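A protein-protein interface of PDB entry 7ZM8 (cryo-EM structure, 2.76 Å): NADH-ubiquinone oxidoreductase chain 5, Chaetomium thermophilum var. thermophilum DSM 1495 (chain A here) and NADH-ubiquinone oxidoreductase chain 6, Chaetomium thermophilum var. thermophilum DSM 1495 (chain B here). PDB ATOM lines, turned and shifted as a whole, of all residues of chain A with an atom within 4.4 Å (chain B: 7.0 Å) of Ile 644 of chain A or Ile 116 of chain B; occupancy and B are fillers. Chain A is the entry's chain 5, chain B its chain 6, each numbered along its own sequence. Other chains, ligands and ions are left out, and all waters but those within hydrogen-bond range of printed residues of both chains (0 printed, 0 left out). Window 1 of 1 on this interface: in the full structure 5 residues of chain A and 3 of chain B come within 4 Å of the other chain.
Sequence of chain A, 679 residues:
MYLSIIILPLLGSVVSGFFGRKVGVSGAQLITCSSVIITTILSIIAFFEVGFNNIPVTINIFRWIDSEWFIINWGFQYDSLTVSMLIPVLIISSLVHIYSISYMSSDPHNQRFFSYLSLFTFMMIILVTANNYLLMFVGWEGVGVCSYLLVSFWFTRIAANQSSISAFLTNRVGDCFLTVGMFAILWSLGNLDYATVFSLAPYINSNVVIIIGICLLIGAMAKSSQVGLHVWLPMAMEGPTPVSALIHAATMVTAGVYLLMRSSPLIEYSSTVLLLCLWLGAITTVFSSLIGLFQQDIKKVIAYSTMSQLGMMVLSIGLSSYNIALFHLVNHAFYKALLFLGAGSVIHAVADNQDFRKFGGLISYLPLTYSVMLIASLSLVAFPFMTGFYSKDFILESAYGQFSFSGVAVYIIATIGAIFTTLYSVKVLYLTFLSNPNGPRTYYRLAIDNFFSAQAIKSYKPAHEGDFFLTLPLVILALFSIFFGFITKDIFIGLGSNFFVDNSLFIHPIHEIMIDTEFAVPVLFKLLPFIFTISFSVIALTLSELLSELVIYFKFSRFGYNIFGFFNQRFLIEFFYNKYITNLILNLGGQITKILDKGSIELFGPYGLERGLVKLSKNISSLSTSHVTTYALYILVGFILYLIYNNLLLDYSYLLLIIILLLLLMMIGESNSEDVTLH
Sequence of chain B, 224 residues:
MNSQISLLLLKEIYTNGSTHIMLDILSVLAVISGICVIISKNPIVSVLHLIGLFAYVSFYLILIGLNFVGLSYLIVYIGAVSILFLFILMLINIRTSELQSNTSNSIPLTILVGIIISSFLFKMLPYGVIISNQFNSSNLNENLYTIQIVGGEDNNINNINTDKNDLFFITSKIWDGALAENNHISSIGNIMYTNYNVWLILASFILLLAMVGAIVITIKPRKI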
ATOM      1  N   ILE A 640      28.886 -28.979 -22.101  1.00  0.00           N
ATOM      2  CA  ILE A 640      27.735 -28.714 -22.957  1.00  0.00           C
ATOM      3  C   ILE A 640      26.938 -29.987 -23.210  1.00  0.00           C
ATOM      4  O   ILE A 640      25.702 -29.964 -23.239  1.00  0.00           O
ATOM      5  CB  ILE A 640      28.191 -28.059 -24.274  1.00  0.00           C
ATOM      6  CG1 ILE A 640      29.001 -26.799 -23.991  1.00  0.00           C
ATOM      7  CG2 ILE A 640      27.004 -27.766 -25.174  1.00  0.00           C
ATOM      8  CD1 ILE A 640      29.885 -26.379 -25.141  1.00  0.00           C
ATOM      9  N   LEU A 641      27.625 -31.112 -23.411  1.00  0.00           N
ATOM     10  CA  LEU A 641      26.918 -32.366 -23.657  1.00  0.00           C
ATOM     11  C   LEU A 641      26.061 -32.771 -22.464  1.00  0.00           C
ATOM     12  O   LEU A 641      24.986 -33.352 -22.637  1.00  0.00           O
ATOM     13  CB  LEU A 641      27.902 -33.478 -24.020  1.00  0.00           C
ATOM     14  CG  LEU A 641      28.364 -33.578 -25.476  1.00  0.00           C
ATOM     15  CD1 LEU A 641      27.170 -33.900 -26.359  1.00  0.00           C
ATOM     16  CD2 LEU A 641      29.062 -32.335 -25.978  1.00  0.00           C
ATOM     17  N   TYR A 642      26.522 -32.485 -21.247  1.00  0.00           N
ATOM     18  CA  TYR A 642      25.685 -32.753 -20.083  1.00  0.00           C
ATOM     19  C   TYR A 642      24.492 -31.809 -20.033  1.00  0.00           C
ATOM     20  O   TYR A 642      23.393 -32.209 -19.638  1.00  0.00           O
ATOM     21  CB  TYR A 642      26.508 -32.657 -18.798  1.00  0.00           C
ATOM     22  CG  TYR A 642      27.300 -33.905 -18.481  1.00  0.00           C
ATOM     23  CD1 TYR A 642      27.582 -34.839 -19.458  1.00  0.00           C
ATOM     24  CD2 TYR A 642      27.764 -34.144 -17.202  1.00  0.00           C
ATOM     25  CE1 TYR A 642      28.302 -35.973 -19.168  1.00  0.00           C
ATOM     26  CE2 TYR A 642      28.481 -35.276 -16.903  1.00  0.00           C
ATOM     27  CZ  TYR A 642      28.747 -36.185 -17.885  1.00  0.00           C
ATOM     28  OH  TYR A 642      29.465 -37.315 -17.591  1.00  0.00           O
ATOM     29  N   LEU A 643      24.692 -30.553 -20.432  1.00  0.00           N
ATOM     30  CA  LEU A 643      23.603 -29.582 -20.422  1.00  0.00           C
ATOM     31  C   LEU A 643      22.549 -29.914 -21.465  1.00  0.00           C
ATOM     32  O   LEU A 643      21.349 -29.786 -21.204  1.00  0.00           O
ATOM     33  CB  LEU A 643      24.152 -28.176 -20.647  1.00  0.00           C
ATOM     34  CG  LEU A 643      24.577 -27.407 -19.401  1.00  0.00           C
ATOM     35  CD1 LEU A 643      23.355 -27.147 -18.576  1.00  0.00           C
ATOM     36  CD2 LEU A 643      25.585 -28.169 -18.580  1.00  0.00           C
ATOM     37  N   ILE A 644      22.977 -30.330 -22.655  1.00  0.00           N
ATOM     38  CA  ILE A 644      22.025 -30.705 -23.695  1.00  0.00           C
ATOM     39  C   ILE A 644      21.214 -31.917 -23.263  1.00  0.00           C
ATOM     40  O   ILE A 644      19.991 -31.956 -23.425  1.00  0.00           O
ATOM     41  CB  ILE A 644      22.762 -30.954 -25.021  1.00  0.00           C
ATOM     42  CG1 ILE A 644      23.228 -29.628 -25.620  1.00  0.00           C
ATOM     43  CG2 ILE A 644      21.879 -31.705 -25.996  1.00  0.00           C
ATOM     44  CD1 ILE A 644      24.118 -29.784 -26.831  1.00  0.00           C
ATOM     45  N   TYR A 645      21.880 -32.919 -22.692  1.00  0.00           N
ATOM     46  CA  TYR A 645      21.200 -34.158 -22.343  1.00  0.00           C
ATOM     47  C   TYR A 645      20.141 -33.936 -21.272  1.00  0.00           C
ATOM     48  O   TYR A 645      19.060 -34.533 -21.325  1.00  0.00           O
ATOM     49  CB  TYR A 645      22.225 -35.195 -21.889  1.00  0.00           C
ATOM     50  CG  TYR A 645      21.627 -36.446 -21.300  1.00  0.00           C
ATOM     51  CD1 TYR A 645      21.334 -37.538 -22.103  1.00  0.00           C
ATOM     52  CD2 TYR A 645      21.376 -36.547 -19.941  1.00  0.00           C
ATOM     53  CE1 TYR A 645      20.792 -38.687 -21.571  1.00  0.00           C
ATOM     54  CE2 TYR A 645      20.835 -37.688 -19.400  1.00  0.00           C
ATOM     55  CZ  TYR A 645      20.546 -38.758 -20.216  1.00  0.00           C
ATOM     56  OH  TYR A 645      20.010 -39.901 -19.675  1.00  0.00           O
ATOM     57  N   ASN A 646      20.425 -33.129 -20.266  1.00  0.00           N
ATOM     58  CA  ASN A 646      19.507 -32.958 -19.109  1.00  0.00           C
ATOM     59  C   ASN A 646      18.660 -31.694 -19.249  1.00  0.00           C
ATOM     60  O   ASN A 646      18.149 -31.227 -18.220  1.00  0.00           O
ATOM     61  CB  ASN A 646      20.293 -32.943 -17.803  1.00  0.00           C
ATOM     62  CG  ASN A 646      19.604 -33.681 -16.677  1.00  0.00           C
ATOM     63  OD1 ASN A 646      18.534 -34.252 -16.865  1.00  0.00           O
ATOM     64  ND2 ASN A 646      20.214 -33.672 -15.504  1.00  0.00           N
ATOM     65  N   ASN A 647      18.475 -31.186 -20.465  1.00  0.00           N
ATOM     66  CA  ASN A 647      17.586 -30.015 -20.675  1.00  0.00           C
ATOM     67  C   ASN A 647      16.751 -30.229 -21.939  1.00  0.00           C
ATOM     68  O   ASN A 647      15.650 -29.652 -22.022  1.00  0.00           O
ATOM     69  CB  ASN A 647      18.357 -28.695 -20.729  1.00  0.00           C
ATOM     70  CG  ASN A 647      18.865 -28.256 -19.373  1.00  0.00           C
ATOM     71  OD1 ASN A 647      18.085 -28.077 -18.441  1.00  0.00           O
ATOM     72  ND2 ASN A 647      20.170 -28.083 -19.255  1.00  0.00           N
ATOM     73  N   LEU A 648      17.254 -31.032 -22.876  1.00  0.00           N
ATOM     74  CA  LEU A 648      16.494 -31.322 -24.118  1.00  0.00           C
ATOM     75  C   LEU A 648      15.645 -32.578 -23.909  1.00  0.00           C
ATOM     76  O   LEU A 648      14.946 -32.968 -24.864  1.00  0.00           O
ATOM     77  CB  LEU A 648      17.466 -31.484 -25.289  1.00  0.00           C
ATOM     78  CG  LEU A 648      17.374 -30.405 -26.366  1.00  0.00           C
ATOM     79  CD1 LEU A 648      17.573 -29.022 -25.767  1.00  0.00           C
ATOM     80  CD2 LEU A 648      18.386 -30.656 -27.473  1.00  0.00           C
ATOM     81  N   LEU A 650      16.253 -35.542 -24.065  1.00  0.00           N
ATOM     82  CA  LEU A 650      16.478 -36.463 -25.205  1.00  0.00           C
ATOM     83  C   LEU A 650      16.271 -37.902 -24.735  1.00  0.00           C
ATOM     84  O   LEU A 650      16.508 -38.170 -23.539  1.00  0.00           O
ATOM     85  CB  LEU A 650      17.906 -36.269 -25.719  1.00  0.00           C
ATOM     86  CG  LEU A 650      18.209 -34.904 -26.329  1.00  0.00           C
ATOM     87  CD1 LEU A 650      19.684 -34.785 -26.676  1.00  0.00           C
ATOM     88  CD2 LEU A 650      17.349 -34.661 -27.558  1.00  0.00           C
ATOM     89  N   ILE B 111      30.097 -19.759 -32.481  1.00  0.00           N
ATOM     90  CA  ILE B 111      28.659 -19.629 -32.695  1.00  0.00           C
ATOM     91  C   ILE B 111      27.910 -20.725 -31.950  1.00  0.00           C
ATOM     92  O   ILE B 111      26.870 -20.476 -31.328  1.00  0.00           O
ATOM     93  CB  ILE B 111      28.340 -19.649 -34.201  1.00  0.00           C
ATOM     94  CG1 ILE B 111      28.935 -18.421 -34.888  1.00  0.00           C
ATOM     95  CG2 ILE B 111      26.841 -19.710 -34.431  1.00  0.00           C
ATOM     96  CD1 ILE B 111      28.978 -18.530 -36.394  1.00  0.00           C
ATOM     97  N   LEU B 112      28.429 -21.952 -31.998  1.00  0.00           N
ATOM     98  CA  LEU B 112      27.752 -23.072 -31.354  1.00  0.00           C
ATOM     99  C   LEU B 112      27.692 -22.891 -29.843  1.00  0.00           C
ATOM    100  O   LEU B 112      26.616 -22.976 -29.239  1.00  0.00           O
ATOM    101  CB  LEU B 112      28.463 -24.375 -31.702  1.00  0.00           C
ATOM    102  CG  LEU B 112      28.317 -24.854 -33.144  1.00  0.00           C
ATOM    103  CD1 LEU B 112      28.866 -26.259 -33.265  1.00  0.00           C
ATOM    104  CD2 LEU B 112      26.866 -24.793 -33.591  1.00  0.00           C
ATOM    105  N   VAL B 113      28.840 -22.635 -29.215  1.00  0.00           N
ATOM    106  CA  VAL B 113      28.888 -22.572 -27.759  1.00  0.00           C
ATOM    107  C   VAL B 113      28.099 -21.374 -27.247  1.00  0.00           C
ATOM    108  O   VAL B 113      27.409 -21.458 -26.225  1.00  0.00           O
ATOM    109  CB  VAL B 113      30.348 -22.544 -27.276  1.00  0.00           C
ATOM    110  CG1 VAL B 113      30.410 -22.360 -25.771  1.00  0.00           C
ATOM    111  CG2 VAL B 113      31.060 -23.822 -27.685  1.00  0.00           C
ATOM    112  N   GLY B 114      28.181 -20.244 -27.950  1.00  0.00           N
ATOM    113  CA  GLY B 114      27.450 -19.065 -27.519  1.00  0.00           C
ATOM    114  C   GLY B 114      25.946 -19.256 -27.553  1.00  0.00           C
ATOM    115  O   GLY B 114      25.231 -18.794 -26.661  1.00  0.00           O
ATOM    116  N   ILE B 115      25.443 -19.932 -28.584  1.00  0.00           N
ATOM    117  CA  ILE B 115      24.001 -20.118 -28.712  1.00  0.00           C
ATOM    118  C   ILE B 115      23.488 -21.075 -27.643  1.00  0.00           C
ATOM    119  O   ILE B 115      22.475 -20.808 -26.984  1.00  0.00           O
ATOM    120  CB  ILE B 115      23.650 -20.608 -30.129  1.00  0.00           C
ATOM    121  CG1 ILE B 115      23.574 -19.425 -31.093  1.00  0.00           C
ATOM    122  CG2 ILE B 115      22.337 -21.374 -30.129  1.00  0.00           C
ATOM    123  CD1 ILE B 115      23.420 -19.829 -32.540  1.00  0.00           C
ATOM    124  N   ILE B 116      24.182 -22.195 -27.445  1.00  0.00           N
ATOM    125  CA  ILE B 116      23.691 -23.222 -26.528  1.00  0.00           C
ATOM    126  C   ILE B 116      23.762 -22.738 -25.085  1.00  0.00           C
ATOM    127  O   ILE B 116      22.801 -22.880 -24.319  1.00  0.00           O
ATOM    128  CB  ILE B 116      24.477 -24.530 -26.721  1.00  0.00           C
ATOM    129  CG1 ILE B 116      24.097 -25.190 -28.045  1.00  0.00           C
ATOM    130  CG2 ILE B 116      24.217 -25.480 -25.566  1.00  0.00           C
ATOM    131  CD1 ILE B 116      25.045 -26.292 -28.468  1.00  0.00           C
ATOM    132  N   ILE B 117      24.897 -22.165 -24.687  1.00  0.00           N
ATOM    133  CA  ILE B 117      25.060 -21.744 -23.300  1.00  0.00           C
ATOM    134  C   ILE B 117      24.080 -20.633 -22.960  1.00  0.00           C
ATOM    135  O   ILE B 117      23.438 -20.656 -21.902  1.00  0.00           O
ATOM    136  CB  ILE B 117      26.515 -21.321 -23.032  1.00  0.00           C
ATOM    137  CG1 ILE B 117      27.410 -22.555 -22.905  1.00  0.00           C
ATOM    138  CG2 ILE B 117      26.602 -20.485 -21.772  1.00  0.00           C
ATOM    139  CD1 ILE B 117      28.813 -22.246 -22.438  1.00  0.00           C
ATOM    140  N   SER B 118      23.943 -19.646 -23.846  1.00  0.00           N
ATOM    141  CA  SER B 118      23.018 -18.551 -23.589  1.00  0.00           C
ATOM    142  C   SER B 118      21.575 -19.038 -23.548  1.00  0.00           C
ATOM    143  O   SER B 118      20.792 -18.608 -22.694  1.00  0.00           O
ATOM    144  CB  SER B 118      23.192 -17.463 -24.645  1.00  0.00           C
ATOM    145  OG  SER B 118      23.093 -18.004 -25.949  1.00  0.00           O
ATOM    146  N   SER B 119      21.206 -19.941 -24.458  1.00  0.00           N
ATOM    147  CA  SER B 119      19.818 -20.386 -24.529  1.00  0.00           C
ATOM    148  C   SER B 119      19.410 -21.197 -23.307  1.00  0.00           C
ATOM    149  O   SER B 119      18.212 -21.357 -23.048  1.00  0.00           O
ATOM    150  CB  SER B 119      19.591 -21.197 -25.803  1.00  0.00           C
ATOM    151  OG  SER B 119      20.400 -22.358 -25.819  1.00  0.00           O
ATOM    152  N   PHE B 120      20.375 -21.717 -22.548  1.00  0.00           N
ATOM    153  CA  PHE B 120      20.050 -22.450 -21.331  1.00  0.00           C
ATOM    154  C   PHE B 120      20.107 -21.561 -20.095  1.00  0.00           C
ATOM    155  O   PHE B 120      19.154 -21.523 -19.311  1.00  0.00           O
ATOM    156  CB  PHE B 120      20.995 -23.642 -21.153  1.00  0.00           C
ATOM    157  CG  PHE B 120      20.645 -24.820 -22.005  1.00  0.00           C
ATOM    158  CD1 PHE B 120      19.418 -24.891 -22.639  1.00  0.00           C
ATOM    159  CD2 PHE B 120      21.540 -25.858 -22.169  1.00  0.00           C
ATOM    160  CE1 PHE B 120      19.095 -25.975 -23.425  1.00  0.00           C
ATOM    161  CE2 PHE B 120      21.223 -26.945 -22.952  1.00  0.00           C
ATOM    162  CZ  PHE B 120      19.999 -27.004 -23.580  1.00  0.00           C
ATOM    163  N   LEU B 121      21.215 -20.841 -19.911  1.00  0.00           N
ATOM    164  CA  LEU B 121      21.392 -20.048 -18.700  1.00  0.00           C
ATOM    165  C   LEU B 121      20.348 -18.948 -18.579  1.00  0.00           C
ATOM    166  O   LEU B 121      19.920 -18.633 -17.466  1.00  0.00           O
ATOM    167  CB  LEU B 121      22.796 -19.452 -18.661  1.00  0.00           C
ATOM    168  CG  LEU B 121      23.865 -20.276 -17.943  1.00  0.00           C
ATOM    169  CD1 LEU B 121      25.262 -19.814 -18.330  1.00  0.00           C
ATOM    170  CD2 LEU B 121      23.672 -20.195 -16.441  1.00  0.00           C
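The backbone carbonyl oxygen of Leu 643 of chain A lies within hydrogen-bond range of the side-chain amide nitrogen of Asn 647 of chain A. The side-chain hydroxyl (OG) of Ser 119 of chain B lies within hydrogen-bond range of the backbone carbonyl oxygen (O) of Ile 116 of chain B (2.9 Å).
Val 113 of chain B touches Ile 640 of chain A. Ile 640 of chain A touches Ile 116 of chain B. Phe 120 of chain B touches Leu 643 of chain A. Ile 644 of chain A touches Ile 116 of chain B (CD1 to CD1, 3.97 Å). Ile 644 of chain A touches Phe 120 of chain B (N to CE2, 3.8 Å). CB of Asn 647 of chain A touches CZ of Phe 120 of chain B, 3.7 Å away. CZ of Phe 120 of chain B touches CD1 of Leu 648 of chain A, at 3.8 Å.
Ile 644 of chain A touches two residues of chain B. Ile 116 of chain B touches just these residues of chain A: Ile 640 (3.6 Å) and Ile 644 (3.97 Å). Printed residues of chain B within 4 Å of Ile 640 of chain A: Val 113 (3.8 Å) and Ile 116 (3.6 Å). Of the printed residues of chain A, Val 113 of chain B touches Ile 640. Of the printed residues of chain B, Asn 647 of chain A touches Phe 120 (3.7 Å). Printed residues of chain A within 4 Å of Phe 120 of chain B: Leu 643, Ile 644, Asn 647 and Leu 648. Of the printed residues of chain B, Leu 648 of chain A touches Phe 120. Tyr 642 of chain A touches none of the printed residues of chain B. Ile 117 of chain B touches none of the printed residues of chain A.
Hydrophobic or aromatic side chains of chain B that line the printed part of chain A: Val 113, Ile 116 and Phe 120. Of the 10 printed residues of chain A, 5 touch a printed residue of chain B. Among the printed residues, no Asp or Glu carboxylate lies within 4 Å of a Lys or Arg side-chain nitrogen of the other chain.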
